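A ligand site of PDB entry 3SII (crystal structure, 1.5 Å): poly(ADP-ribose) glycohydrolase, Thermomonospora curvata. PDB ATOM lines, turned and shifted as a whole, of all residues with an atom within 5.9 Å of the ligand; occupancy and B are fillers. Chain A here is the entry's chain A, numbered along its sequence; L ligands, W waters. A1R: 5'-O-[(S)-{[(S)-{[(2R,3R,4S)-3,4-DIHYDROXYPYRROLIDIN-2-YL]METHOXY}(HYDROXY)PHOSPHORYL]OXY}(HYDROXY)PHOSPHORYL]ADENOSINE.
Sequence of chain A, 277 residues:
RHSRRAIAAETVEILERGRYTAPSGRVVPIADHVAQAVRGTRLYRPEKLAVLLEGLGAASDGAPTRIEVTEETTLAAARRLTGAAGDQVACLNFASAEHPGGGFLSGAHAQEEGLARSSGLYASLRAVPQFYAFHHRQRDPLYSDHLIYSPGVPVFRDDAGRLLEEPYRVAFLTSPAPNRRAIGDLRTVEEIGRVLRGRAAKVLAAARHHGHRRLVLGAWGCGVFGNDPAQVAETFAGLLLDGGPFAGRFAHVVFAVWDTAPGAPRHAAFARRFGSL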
ATOM      1  N   GLU A  72      22.944  -6.133 -12.215  1.00  0.00           N
ATOM      2  CA  GLU A  72      21.605  -6.190 -11.657  1.00  0.00           C
ATOM      3  C   GLU A  72      21.610  -6.256 -10.137  1.00  0.00           C
ATOM      4  O   GLU A  72      22.516  -6.840  -9.522  1.00  0.00           O
ATOM      5  CB  GLU A  72      20.884  -7.424 -12.178  1.00  0.00           C
ATOM      6  CG  GLU A  72      20.484  -7.377 -13.636  1.00  0.00           C
ATOM      7  CD  GLU A  72      20.019  -8.733 -14.134  1.00  0.00           C
ATOM      8  OE1 GLU A  72      20.758  -9.719 -13.941  1.00  0.00           O
ATOM      9  OE2 GLU A  72      18.905  -8.815 -14.701  1.00  0.00           O
ATOM     10  N   THR A  73      20.579  -5.698  -9.516  1.00  0.00           N
ATOM     11  CA  THR A  73      20.268  -6.042  -8.134  1.00  0.00           C
ATOM     12  C   THR A  73      19.828  -7.507  -8.073  1.00  0.00           C
ATOM     13  O   THR A  73      19.418  -8.111  -9.069  1.00  0.00           O
ATOM     14  CB  THR A  73      19.122  -5.200  -7.565  1.00  0.00           C
ATOM     15  OG1 THR A  73      17.917  -5.465  -8.310  1.00  0.00           O
ATOM     16  CG2 THR A  73      19.449  -3.713  -7.635  1.00  0.00           C
ATOM     17  N   THR A  74      19.945  -8.088  -6.882  1.00  0.00           N
ATOM     18  CA  THR A  74      19.442  -9.422  -6.624  1.00  0.00           C
ATOM     19  C   THR A  74      18.005  -9.587  -7.132  1.00  0.00           C
ATOM     20  O   THR A  74      17.689 -10.533  -7.866  1.00  0.00           O
ATOM     21  CB  THR A  74      19.465  -9.730  -5.114  1.00  0.00           C
ATOM     22  OG1 THR A  74      20.778  -9.449  -4.598  1.00  0.00           O
ATOM     23  CG2 THR A  74      19.111 -11.195  -4.842  1.00  0.00           C
ATOM     24  N   LEU A  75      17.127  -8.665  -6.744  1.00  0.00           N
ATOM     25  CA  LEU A  75      15.729  -8.782  -7.164  1.00  0.00           C
ATOM     26  C   LEU A  75      15.526  -8.584  -8.664  1.00  0.00           C
ATOM     27  O   LEU A  75      14.667  -9.253  -9.254  1.00  0.00           O
ATOM     28  CB  LEU A  75      14.854  -7.821  -6.363  1.00  0.00           C
ATOM     29  CG  LEU A  75      14.649  -8.274  -4.913  1.00  0.00           C
ATOM     30  CD1 LEU A  75      13.710  -7.331  -4.187  1.00  0.00           C
ATOM     31  CD2 LEU A  75      14.143  -9.705  -4.848  1.00  0.00           C
ATOM     32  N   PHE A  94      22.146 -11.814   1.723  1.00  0.00           N
ATOM     33  CA  PHE A  94      23.413 -11.498   2.390  1.00  0.00           C
ATOM     34  C   PHE A  94      23.070 -11.083   3.820  1.00  0.00           C
ATOM     35  O   PHE A  94      22.974  -9.888   4.150  1.00  0.00           O
ATOM     36  CB  PHE A  94      24.149 -10.354   1.675  1.00  0.00           C
ATOM     37  CG  PHE A  94      24.382 -10.574   0.193  1.00  0.00           C
ATOM     38  CD1 PHE A  94      24.329 -11.841  -0.379  1.00  0.00           C
ATOM     39  CD2 PHE A  94      24.710  -9.490  -0.618  1.00  0.00           C
ATOM     40  CE1 PHE A  94      24.558 -12.020  -1.741  1.00  0.00           C
ATOM     41  CE2 PHE A  94      24.951  -9.662  -1.977  1.00  0.00           C
ATOM     42  CZ  PHE A  94      24.868 -10.938  -2.538  1.00  0.00           C
ATOM     43  N   ALA A  95      22.892 -12.092   4.660  1.00  0.00           N
ATOM     44  CA  ALA A  95      22.118 -11.957   5.885  1.00  0.00           C
ATOM     45  C   ALA A  95      22.867 -11.359   7.050  1.00  0.00           C
ATOM     46  O   ALA A  95      24.070 -11.595   7.233  1.00  0.00           O
ATOM     47  CB  ALA A  95      21.568 -13.303   6.290  1.00  0.00           C
ATOM     48  N   SER A  96      22.125 -10.607   7.865  1.00  0.00           N
ATOM     49  CA  SER A  96      22.529 -10.331   9.230  1.00  0.00           C
ATOM     50  C   SER A  96      22.418 -11.610  10.042  1.00  0.00           C
ATOM     51  O   SER A  96      21.470 -12.395   9.869  1.00  0.00           O
ATOM     52  CB  SER A  96      21.616  -9.278   9.832  1.00  0.00           C
ATOM     53  OG  SER A  96      21.862  -9.117  11.230  1.00  0.00           O
ATOM     54  N   ALA A  97      23.378 -11.832  10.930  1.00  0.00           N
ATOM     55  CA  ALA A  97      23.325 -12.971  11.826  1.00  0.00           C
ATOM     56  C   ALA A  97      22.405 -12.695  12.996  1.00  0.00           C
ATOM     57  O   ALA A  97      21.947 -13.621  13.663  1.00  0.00           O
ATOM     58  CB  ALA A  97      24.719 -13.272  12.343  1.00  0.00           C
ATOM     59  N   HIS A  99      19.726  -9.841  13.237  1.00  0.00           N
ATOM     60  CA  HIS A  99      18.404  -9.246  13.079  1.00  0.00           C
ATOM     61  C   HIS A  99      17.769  -9.622  11.759  1.00  0.00           C
ATOM     62  O   HIS A  99      18.375  -9.420  10.697  1.00  0.00           O
ATOM     63  CB  HIS A  99      18.493  -7.711  13.158  1.00  0.00           C
ATOM     64  CG  HIS A  99      19.079  -7.203  14.441  1.00  0.00           C
ATOM     65  ND1 HIS A  99      20.366  -6.715  14.532  1.00  0.00           N
ATOM     66  CD2 HIS A  99      18.556  -7.145  15.686  1.00  0.00           C
ATOM     67  CE1 HIS A  99      20.605  -6.351  15.777  1.00  0.00           C
ATOM     68  NE2 HIS A  99      19.530  -6.603  16.501  1.00  0.00           N
ATOM     69  N   GLY A 101      16.109  -9.284   8.474  1.00  0.00           N
ATOM     70  CA  GLY A 101      15.978  -8.124   7.608  1.00  0.00           C
ATOM     71  C   GLY A 101      16.967  -7.008   7.956  1.00  0.00           C
ATOM     72  O   GLY A 101      16.865  -5.877   7.457  1.00  0.00           O
ATOM     73  N   GLY A 102      17.916  -7.313   8.829  1.00  0.00           N
ATOM     74  CA  GLY A 102      18.941  -6.352   9.177  1.00  0.00           C
ATOM     75  C   GLY A 102      18.324  -5.105   9.784  1.00  0.00           C
ATOM     76  O   GLY A 102      17.449  -5.197  10.636  1.00  0.00           O
ATOM     77  N   GLY A 103      18.785  -3.949   9.338  1.00  0.00           N
ATOM     78  CA  GLY A 103      18.270  -2.701   9.872  1.00  0.00           C
ATOM     79  C   GLY A 103      17.205  -2.065   9.003  1.00  0.00           C
ATOM     80  O   GLY A 103      17.071  -0.849   8.985  1.00  0.00           O
ATOM     81  N   ALA A 110      21.240  -1.744   2.480  1.00  0.00           N
ATOM     82  CA  ALA A 110      22.128  -2.836   2.100  1.00  0.00           C
ATOM     83  C   ALA A 110      21.279  -3.904   1.408  1.00  0.00           C
ATOM     84  O   ALA A 110      20.066  -3.728   1.266  1.00  0.00           O
ATOM     85  CB  ALA A 110      22.853  -3.406   3.314  1.00  0.00           C
ATOM     86  N   GLN A 111      21.891  -4.990   0.951  1.00  0.00           N
ATOM     87  CA  GLN A 111      21.139  -5.945   0.134  1.00  0.00           C
ATOM     88  C   GLN A 111      19.965  -6.591   0.881  1.00  0.00           C
ATOM     89  O   GLN A 111      18.839  -6.666   0.359  1.00  0.00           O
ATOM     90  CB  GLN A 111      22.075  -6.999  -0.460  1.00  0.00           C
ATOM     91  CG  GLN A 111      21.404  -7.914  -1.467  1.00  0.00           C
ATOM     92  CD  GLN A 111      21.196  -9.323  -0.937  1.00  0.00           C
ATOM     93  OE1 GLN A 111      21.178  -9.542   0.279  1.00  0.00           O
ATOM     94  NE2 GLN A 111      21.052 -10.290  -1.839  1.00  0.00           N
ATOM     95  N   GLU A 112      20.208  -7.064   2.101  1.00  0.00           N
ATOM     96  CA  GLU A 112      19.142  -7.733   2.849  1.00  0.00           C
ATOM     97  C   GLU A 112      17.978  -6.790   3.128  1.00  0.00           C
ATOM     98  O   GLU A 112      16.808  -7.163   3.010  1.00  0.00           O
ATOM     99  CB  GLU A 112      19.650  -8.326   4.159  1.00  0.00           C
ATOM    100  CG  GLU A 112      18.487  -8.882   4.996  1.00  0.00           C
ATOM    101  CD  GLU A 112      18.921  -9.638   6.237  1.00  0.00           C
ATOM    102  OE1 GLU A 112      19.950  -9.284   6.832  1.00  0.00           O
ATOM    103  OE2 GLU A 112      18.180 -10.565   6.635  1.00  0.00           O
ATOM    104  N   GLU A 113      18.310  -5.566   3.532  1.00  0.00           N
ATOM    105  CA  GLU A 113      17.294  -4.569   3.821  1.00  0.00           C
ATOM    106  C   GLU A 113      16.395  -4.322   2.600  1.00  0.00           C
ATOM    107  O   GLU A 113      15.171  -4.201   2.736  1.00  0.00           O
ATOM    108  CB  GLU A 113      17.951  -3.265   4.290  1.00  0.00           C
ATOM    109  CG  GLU A 113      18.461  -3.328   5.721  1.00  0.00           C
ATOM    110  CD  GLU A 113      19.872  -3.873   5.869  1.00  0.00           C
ATOM    111  OE1 GLU A 113      20.391  -4.495   4.919  1.00  0.00           O
ATOM    112  OE2 GLU A 113      20.464  -3.689   6.953  1.00  0.00           O
ATOM    113  N   ALA A 177      27.567 -14.243   5.902  1.00  0.00           N
ATOM    114  CA  ALA A 177      28.995 -14.348   5.668  1.00  0.00           C
ATOM    115  C   ALA A 177      29.718 -13.977   6.962  1.00  0.00           C
ATOM    116  O   ALA A 177      29.164 -13.256   7.797  1.00  0.00           O
ATOM    117  CB  ALA A 177      29.418 -13.410   4.541  1.00  0.00           C
ATOM    118  N   GLY A 218      25.978 -13.448  -5.559  1.00  0.00           N
ATOM    119  CA  GLY A 218      26.580 -12.126  -5.674  1.00  0.00           C
ATOM    120  C   GLY A 218      27.706 -11.945  -4.686  1.00  0.00           C
ATOM    121  O   GLY A 218      28.281 -12.951  -4.224  1.00  0.00           O
ATOM    122  N   ALA A 219      28.017 -10.687  -4.384  1.00  0.00           N
ATOM    123  CA  ALA A 219      29.158 -10.313  -3.550  1.00  0.00           C
ATOM    124  C   ALA A 219      28.850 -10.413  -2.060  1.00  0.00           C
ATOM    125  O   ALA A 219      28.991  -9.453  -1.291  1.00  0.00           O
ATOM    126  CB  ALA A 219      29.658  -8.908  -3.929  1.00  0.00           C
ATOM    127  N   TRP A 220      28.380 -11.604  -1.690  1.00  0.00           N
ATOM    128  CA  TRP A 220      28.109 -12.003  -0.326  1.00  0.00           C
ATOM    129  C   TRP A 220      29.206 -11.543   0.637  1.00  0.00           C
ATOM    130  O   TRP A 220      30.382 -11.850   0.443  1.00  0.00           O
ATOM    131  CB  TRP A 220      28.054 -13.534  -0.343  1.00  0.00           C
ATOM    132  CG  TRP A 220      27.583 -14.256   0.895  1.00  0.00           C
ATOM    133  CD1 TRP A 220      26.567 -13.904   1.749  1.00  0.00           C
ATOM    134  CD2 TRP A 220      28.132 -15.480   1.386  1.00  0.00           C
ATOM    135  NE1 TRP A 220      26.448 -14.867   2.737  1.00  0.00           N
ATOM    136  CE2 TRP A 220      27.395 -15.839   2.531  1.00  0.00           C
ATOM    137  CE3 TRP A 220      29.176 -16.314   0.952  1.00  0.00           C
ATOM    138  CZ2 TRP A 220      27.678 -16.993   3.263  1.00  0.00           C
ATOM    139  CZ3 TRP A 220      29.451 -17.448   1.674  1.00  0.00           C
ATOM    140  CH2 TRP A 220      28.711 -17.785   2.817  1.00  0.00           C
ATOM    141  N   GLY A 221      28.809 -10.789   1.653  1.00  0.00           N
ATOM    142  CA  GLY A 221      29.742 -10.390   2.706  1.00  0.00           C
ATOM    143  C   GLY A 221      30.740  -9.296   2.332  1.00  0.00           C
ATOM    144  O   GLY A 221      31.608  -8.961   3.145  1.00  0.00           O
ATOM    145  N   CYS A 222      30.599  -8.718   1.147  1.00  0.00           N
ATOM    146  CA  CYS A 222      31.628  -7.808   0.633  1.00  0.00           C
ATOM    147  C   CYS A 222      31.320  -6.328   0.831  1.00  0.00           C
ATOM    148  O   CYS A 222      32.049  -5.476   0.318  1.00  0.00           O
ATOM    149  CB  CYS A 222      31.897  -8.101  -0.851  1.00  0.00           C
ATOM    150  SG  CYS A 222      32.613  -9.721  -1.145  1.00  0.00           S
ATOM    151  N   GLY A 223      30.251  -6.046   1.561  1.00  0.00           N
ATOM    152  CA  GLY A 223      29.900  -4.678   1.896  1.00  0.00           C
ATOM    153  C   GLY A 223      30.261  -4.396   3.340  1.00  0.00           C
ATOM    154  O   GLY A 223      31.428  -4.320   3.697  1.00  0.00           O
ATOM    155  N   VAL A 224      29.234  -4.290   4.182  1.00  0.00           N
ATOM    156  CA  VAL A 224      29.413  -4.018   5.596  1.00  0.00           C
ATOM    157  C   VAL A 224      30.350  -5.024   6.258  1.00  0.00           C
ATOM    158  O   VAL A 224      31.112  -4.672   7.156  1.00  0.00           O
ATOM    159  CB  VAL A 224      28.061  -4.040   6.330  1.00  0.00           C
ATOM    160  CG1 VAL A 224      28.258  -3.677   7.792  1.00  0.00           C
ATOM    161  CG2 VAL A 224      27.075  -3.094   5.664  1.00  0.00           C
ATOM    162  N   PHE A 225      30.278  -6.275   5.822  1.00  0.00           N
ATOM    163  CA  PHE A 225      31.072  -7.350   6.449  1.00  0.00           C
ATOM    164  C   PHE A 225      32.530  -7.379   5.995  1.00  0.00           C
ATOM    165  O   PHE A 225      33.321  -8.126   6.545  1.00  0.00           O
ATOM    166  CB  PHE A 225      30.404  -8.715   6.234  1.00  0.00           C
ATOM    167  CG  PHE A 225      29.234  -8.978   7.139  1.00  0.00           C
ATOM    168  CD1 PHE A 225      28.829  -8.050   8.082  1.00  0.00           C
ATOM    169  CD2 PHE A 225      28.523 -10.172   7.039  1.00  0.00           C
ATOM    170  CE1 PHE A 225      27.751  -8.293   8.917  1.00  0.00           C
ATOM    171  CE2 PHE A 225      27.433 -10.421   7.872  1.00  0.00           C
ATOM    172  CZ  PHE A 225      27.047  -9.482   8.811  1.00  0.00           C
ATOM    173  N   GLY A 226      32.854  -6.568   4.996  1.00  0.00           N
ATOM    174  CA  GLY A 226      34.243  -6.327   4.621  1.00  0.00           C
ATOM    175  C   GLY A 226      35.037  -7.503   4.073  1.00  0.00           C
ATOM    176  O   GLY A 226      36.263  -7.552   4.197  1.00  0.00           O
ATOM    177  N   ASN A 227      34.366  -8.458   3.459  1.00  0.00           N
ATOM    178  CA  ASN A 227      35.097  -9.528   2.803  1.00  0.00           C
ATOM    179  C   ASN A 227      35.711  -9.048   1.491  1.00  0.00           C
ATOM    180  O   ASN A 227      35.278  -8.047   0.928  1.00  0.00           O
ATOM    181  CB  ASN A 227      34.210 -10.763   2.562  1.00  0.00           C
ATOM    182  CG  ASN A 227      34.006 -11.576   3.810  1.00  0.00           C
ATOM    183  OD1 ASN A 227      34.825 -12.417   4.170  1.00  0.00           O
ATOM    184  ND2 ASN A 227      32.894 -11.320   4.501  1.00  0.00           N
ATOM    185  N   ALA A 256      24.643 -11.384  -9.584  1.00  0.00           N
ATOM    186  CA  ALA A 256      24.045 -10.056  -9.723  1.00  0.00           C
ATOM    187  C   ALA A 256      24.712  -9.158  -8.699  1.00  0.00           C
ATOM    188  O   ALA A 256      24.480  -9.282  -7.496  1.00  0.00           O
ATOM    189  CB  ALA A 256      22.539 -10.129  -9.503  1.00  0.00           C
ATOM    190  N   VAL A 257      25.553  -8.250  -9.190  1.00  0.00           N
ATOM    191  CA  VAL A 257      26.351  -7.412  -8.312  1.00  0.00           C
ATOM    192  C   VAL A 257      26.117  -5.949  -8.647  1.00  0.00           C
ATOM    193  O   VAL A 257      26.664  -5.404  -9.624  1.00  0.00           O
ATOM    194  CB  VAL A 257      27.852  -7.750  -8.411  1.00  0.00           C
ATOM    195  CG1 VAL A 257      28.615  -6.985  -7.334  1.00  0.00           C
ATOM    196  CG2 VAL A 257      28.074  -9.264  -8.295  1.00  0.00           C
ATOM    197  N   TRP A 258      25.278  -5.308  -7.830  1.00  0.00           N
ATOM    198  CA  TRP A 258      24.929  -3.905  -7.962  1.00  0.00           C
ATOM    199  C   TRP A 258      25.774  -3.114  -6.960  1.00  0.00           C
ATOM    200  O   TRP A 258      25.510  -3.138  -5.763  1.00  0.00           O
ATOM    201  CB  TRP A 258      23.448  -3.706  -7.655  1.00  0.00           C
ATOM    202  CG  TRP A 258      23.007  -2.276  -7.713  1.00  0.00           C
ATOM    203  CD1 TRP A 258      23.068  -1.449  -8.798  1.00  0.00           C
ATOM    204  CD2 TRP A 258      22.441  -1.506  -6.654  1.00  0.00           C
ATOM    205  NE1 TRP A 258      22.576  -0.211  -8.478  1.00  0.00           N
ATOM    206  CE2 TRP A 258      22.182  -0.217  -7.153  1.00  0.00           C
ATOM    207  CE3 TRP A 258      22.126  -1.773  -5.318  1.00  0.00           C
ATOM    208  CZ2 TRP A 258      21.631   0.797  -6.381  1.00  0.00           C
ATOM    209  CZ3 TRP A 258      21.569  -0.763  -4.540  1.00  0.00           C
ATOM    210  CH2 TRP A 258      21.331   0.511  -5.078  1.00  0.00           C
ATOM    211  N   ASP A 259      26.800  -2.425  -7.473  1.00  0.00           N
ATOM    212  CA  ASP A 259      27.789  -1.766  -6.627  1.00  0.00           C
ATOM    213  C   ASP A 259      27.861  -0.299  -7.020  1.00  0.00           C
ATOM    214  O   ASP A 259      28.377   0.040  -8.090  1.00  0.00           O
ATOM    215  CB  ASP A 259      29.161  -2.420  -6.817  1.00  0.00           C
ATOM    216  CG  ASP A 259      30.204  -1.924  -5.834  1.00  0.00           C
ATOM    217  OD1 ASP A 259      29.908  -0.966  -5.074  1.00  0.00           O
ATOM    218  OD2 ASP A 259      31.310  -2.502  -5.810  1.00  0.00           O
ATOM    219  N   THR A 260      27.357   0.570  -6.158  1.00  0.00           N
ATOM    220  CA  THR A 260      27.280   1.989  -6.486  1.00  0.00           C
ATOM    221  C   THR A 260      28.553   2.762  -6.148  1.00  0.00           C
ATOM    222  O   THR A 260      28.658   3.951  -6.456  1.00  0.00           O
ATOM    223  CB  THR A 260      26.063   2.652  -5.800  1.00  0.00           C
ATOM    224  OG1 THR A 260      26.208   2.568  -4.377  1.00  0.00           O
ATOM    225  CG2 THR A 260      24.770   1.969  -6.227  1.00  0.00           C
ATOM    226  N   ARG A 266      33.266  -4.463  -6.413  1.00  0.00           N
ATOM    227  CA  ARG A 266      32.701  -5.776  -6.139  1.00  0.00           C
ATOM    228  C   ARG A 266      32.293  -6.437  -7.450  1.00  0.00           C
ATOM    229  O   ARG A 266      32.536  -7.636  -7.661  1.00  0.00           O
ATOM    230  CB  ARG A 266      31.467  -5.631  -5.243  1.00  0.00           C
ATOM    231  CG  ARG A 266      31.728  -5.785  -3.743  1.00  0.00           C
ATOM    232  CD  ARG A 266      32.562  -4.681  -3.144  1.00  0.00           C
ATOM    233  NE  ARG A 266      31.976  -3.353  -3.305  1.00  0.00           N
ATOM    234  CZ  ARG A 266      31.786  -2.495  -2.306  1.00  0.00           C
ATOM    235  NH1 ARG A 266      32.075  -2.843  -1.066  1.00  0.00           N
ATOM    236  NH2 ARG A 266      31.281  -1.278  -2.555  1.00  0.00           N
ATOM    237  N   HIS A 267      31.643  -5.671  -8.315  1.00  0.00           N
ATOM    238  CA  HIS A 267      31.267  -6.187  -9.623  1.00  0.00           C
ATOM    239  C   HIS A 267      32.487  -6.508 -10.491  1.00  0.00           C
ATOM    240  O   HIS A 267      32.522  -7.547 -11.151  1.00  0.00           O
ATOM    241  CB  HIS A 267      30.372  -5.191 -10.351  1.00  0.00           C
ATOM    242  CG  HIS A 267      30.095  -5.573 -11.764  1.00  0.00           C
ATOM    243  ND1 HIS A 267      30.870  -5.130 -12.825  1.00  0.00           N
ATOM    244  CD2 HIS A 267      29.155  -6.387 -12.309  1.00  0.00           C
ATOM    245  CE1 HIS A 267      30.407  -5.642 -13.948  1.00  0.00           C
ATOM    246  NE2 HIS A 267      29.371  -6.413 -13.662  1.00  0.00           N
HETATM  247  N1  A1R L   1      21.827  -6.477  -5.232  1.00  0.00           N
HETATM  248  C2  A1R L   1      23.034  -6.977  -5.628  1.00  0.00           C
HETATM  249  N3  A1R L   1      24.202  -6.561  -5.081  1.00  0.00           N
HETATM  250  C4  A1R L   1      24.065  -5.638  -4.143  1.00  0.00           C
HETATM  251  C5  A1R L   1      22.893  -5.071  -3.647  1.00  0.00           C
HETATM  252  C6  A1R L   1      21.748  -5.543  -4.251  1.00  0.00           C
HETATM  253  N6  A1R L   1      20.459  -5.046  -3.883  1.00  0.00           N
HETATM  254  N7  A1R L   1      23.186  -4.147  -2.657  1.00  0.00           N
HETATM  255  C8  A1R L   1      24.522  -4.161  -2.531  1.00  0.00           C
HETATM  256  N9  A1R L   1      25.119  -5.044  -3.419  1.00  0.00           N
HETATM  257  C1' A1R L   1      26.521  -5.353  -3.577  1.00  0.00           C
HETATM  258  C2' A1R L   1      27.450  -4.268  -3.130  1.00  0.00           C
HETATM  259  O2' A1R L   1      28.579  -4.233  -3.943  1.00  0.00           O
HETATM  260  C3' A1R L   1      27.815  -4.664  -1.751  1.00  0.00           C
HETATM  261  O3' A1R L   1      29.081  -4.220  -1.402  1.00  0.00           O
HETATM  262  O4' A1R L   1      26.859  -6.484  -2.812  1.00  0.00           O
HETATM  263  C4' A1R L   1      27.779  -6.151  -1.814  1.00  0.00           C
HETATM  264  C5' A1R L   1      27.442  -6.767  -0.466  1.00  0.00           C
HETATM  265  O5' A1R L   1      26.223  -6.289   0.004  1.00  0.00           O
HETATM  266  PA  A1R L   1      25.966  -6.101   1.571  1.00  0.00           P
HETATM  267  O1A A1R L   1      24.477  -5.920   1.675  1.00  0.00           O
HETATM  268  O2A A1R L   1      26.746  -4.997   2.195  1.00  0.00           O
HETATM  269  O3A A1R L   1      26.326  -7.513   2.191  1.00  0.00           O
HETATM  270  PB  A1R L   1      27.199  -7.883   3.489  1.00  0.00           P
HETATM  271  O1B A1R L   1      28.635  -7.421   3.378  1.00  0.00           O
HETATM  272  O2B A1R L   1      27.098  -9.369   3.633  1.00  0.00           O
HETATM  273  O5N A1R L   1      26.590  -7.091   4.711  1.00  0.00           O
HETATM  274  C5N A1R L   1      25.529  -7.607   5.456  1.00  0.00           C
HETATM  275  N4N A1R L   1      24.380  -5.946   5.767  1.00  0.00           N
HETATM  276  C1N A1R L   1      22.923  -5.938   5.741  1.00  0.00           C
HETATM  277  O2N A1R L   1      21.482  -7.007   7.283  1.00  0.00           O
HETATM  278  C2N A1R L   1      22.504  -7.209   6.387  1.00  0.00           C
HETATM  279  O3N A1R L   1      24.066  -7.096   8.179  1.00  0.00           O
HETATM  280  C3N A1R L   1      23.757  -7.731   6.991  1.00  0.00           C
HETATM  281  C4N A1R L   1      25.011  -7.158   6.509  1.00  0.00           C
HETATM  282  O   HOH W   1      28.771  -1.916  -0.333  1.00  0.00           O
HETATM  283  O   HOH W   2      22.430  -6.458  11.054  1.00  0.00           O
HETATM  284  O   HOH W   3      26.042  -8.865  -5.246  1.00  0.00           O
HETATM  285  O   HOH W   4      17.949  -5.734  -2.061  1.00  0.00           O
HETATM  286  O   HOH W   5      26.515  -2.394   2.314  1.00  0.00           O
HETATM  287  O   HOH W   6      25.598  -2.102  -0.155  1.00  0.00           O
HETATM  288  O   HOH W   7      25.140  -4.562   7.910  1.00  0.00           O
HETATM  289  O   HOH W   8      21.762  -2.170  -1.296  1.00  0.00           O
HETATM  290  O   HOH W   9      22.877  -7.292   3.157  1.00  0.00           O
HETATM  291  O   HOH W  10      17.708  -6.335  -4.816  1.00  0.00           O
HETATM  292  O   HOH W  11      26.144 -11.856   4.925  1.00  0.00           O
HETATM  293  O   HOH W  12      19.156  -3.055  -2.027  1.00  0.00           O
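The backbone NH of Phe 225 lies within hydrogen-bond range of an oxygen (O1B) of the ligand (3.2 Å).
N of Cys 222 lies within hydrogen-bond range of O1B of the ligand, at 3.2 Å.
N of Thr 74 sits at hydrogen-bond distance from N1 of the ligand (3.0 Å).
OG1 of Thr 74 is in hydrogen-bond range of N1 of the ligand, 3.2 Å away.
The backbone NH (N) of Gln 111 lies within hydrogen-bond range of an oxygen (O1A) of the ligand (2.8 Å).
O3' of the ligand sits at hydrogen-bond distance from NH1 of Arg 266.
The backbone NH (N) of Gly 223 is in hydrogen-bond range of an oxygen (O1B) of the ligand, 2.8 Å away.
The backbone NH of Trp 258 lies within hydrogen-bond range of a nitrogen (N3) of the ligand, 3.2 Å away.
OE2 of Glu 113 sits at hydrogen-bond distance from O2N of the ligand, at 3.5 Å.
O2A of the ligand lies within hydrogen-bond range of N of Val 224 (3.3 Å).
The backbone NH (N) of Gly 221 sits at hydrogen-bond distance from an oxygen (O2B) of the ligand, 3.0 Å away.
An oxygen (O2N) of the ligand is in hydrogen-bond range of the side-chain carboxylate (OE1) of Glu 112 (2.8 Å).
The side-chain carboxylate (OE2) of Glu 112 lies within hydrogen-bond range of the backbone NH (N) of Gly 101, 3.1 Å away.
The guanidinium group (NE) of Arg 266 is in salt-bridge range of the side-chain carboxylate (OD2) of Asp 259, 2.7 Å away.
The guanidinium group of Arg 266 sits at hydrogen-bond distance from the backbone carbonyl oxygen of Cys 222, at 3.0 Å.
The side-chain hydroxyl (OG1) of Thr 74 is in hydrogen-bond range of the side-chain amide nitrogen (NE2) of Gln 111.
The backbone NH (N) of Phe 94 lies within hydrogen-bond range of the side-chain amide oxygen (OE1) of Gln 111, at 2.9 Å.
The side-chain sulfur (SG) of Cys 222 is in hydrogen-bond range of the backbone carbonyl oxygen (O) of Trp 220 (3.5 Å).
OE1 of Glu 112 sits at hydrogen-bond distance from N of Ser 96, 2.7 Å away.
The backbone carbonyl oxygen (O) of Gly 221 sits at hydrogen-bond distance from the backbone NH (N) of Asn 227 (2.8 Å).
Merely in contact with the ligand: Ala 219 (3.2 Å), Gly 102 (3.2 Å), Ala 256 (3.3 Å), Thr 73 (3.3 Å), Asp 259 (3.4 Å), Ala 110 (3.4 Å), Ser 96 (3.4 Å), Phe 94 (3.5 Å), Ala 95 (3.7 Å), Glu 72 (3.9 Å) and Val 257 (3.97 Å).
Within 4 Å of the ligand: Glu 72, Thr 73, Thr 74, Phe 94, Ala 95, Ser 96, Gly 102, Ala 110, Gln 111, Glu 112, Glu 113, Ala 219, Gly 221, Cys 222, Gly 223, Val 224, Phe 225, Ala 256, Val 257, Trp 258, Asp 259 and Arg 266.
Along chain A the residues within 4 Å of the ligand span positions 72 to 266.
The nearest printed residue that does not touch the ligand is Trp 220 (4.3 Å).
Water W1 lies within hydrogen-bond range of an oxygen (O3') of the ligand (2.6 Å) and the guanidinium group of Arg 266 (3.4 Å).
Water W8 lies within hydrogen-bond range of a nitrogen (N7) of the ligand and the backbone carbonyl oxygen (O) of Ala 110.
Water W12 bridges N6 of the ligand (3.0 Å) and O of Ala 110 (3.5 Å).
Water W4 bridges O of Gln 111 (2.7 Å) and N6 of the ligand (3.2 Å).
Water W10 lies within hydrogen-bond range of N of Leu 75 and N6 of the ligand.
Water W2 bridges the side-chain hydroxyl (OG) of Ser 96 (2.7 Å) and an oxygen (O3N) of the ligand (3.4 Å).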
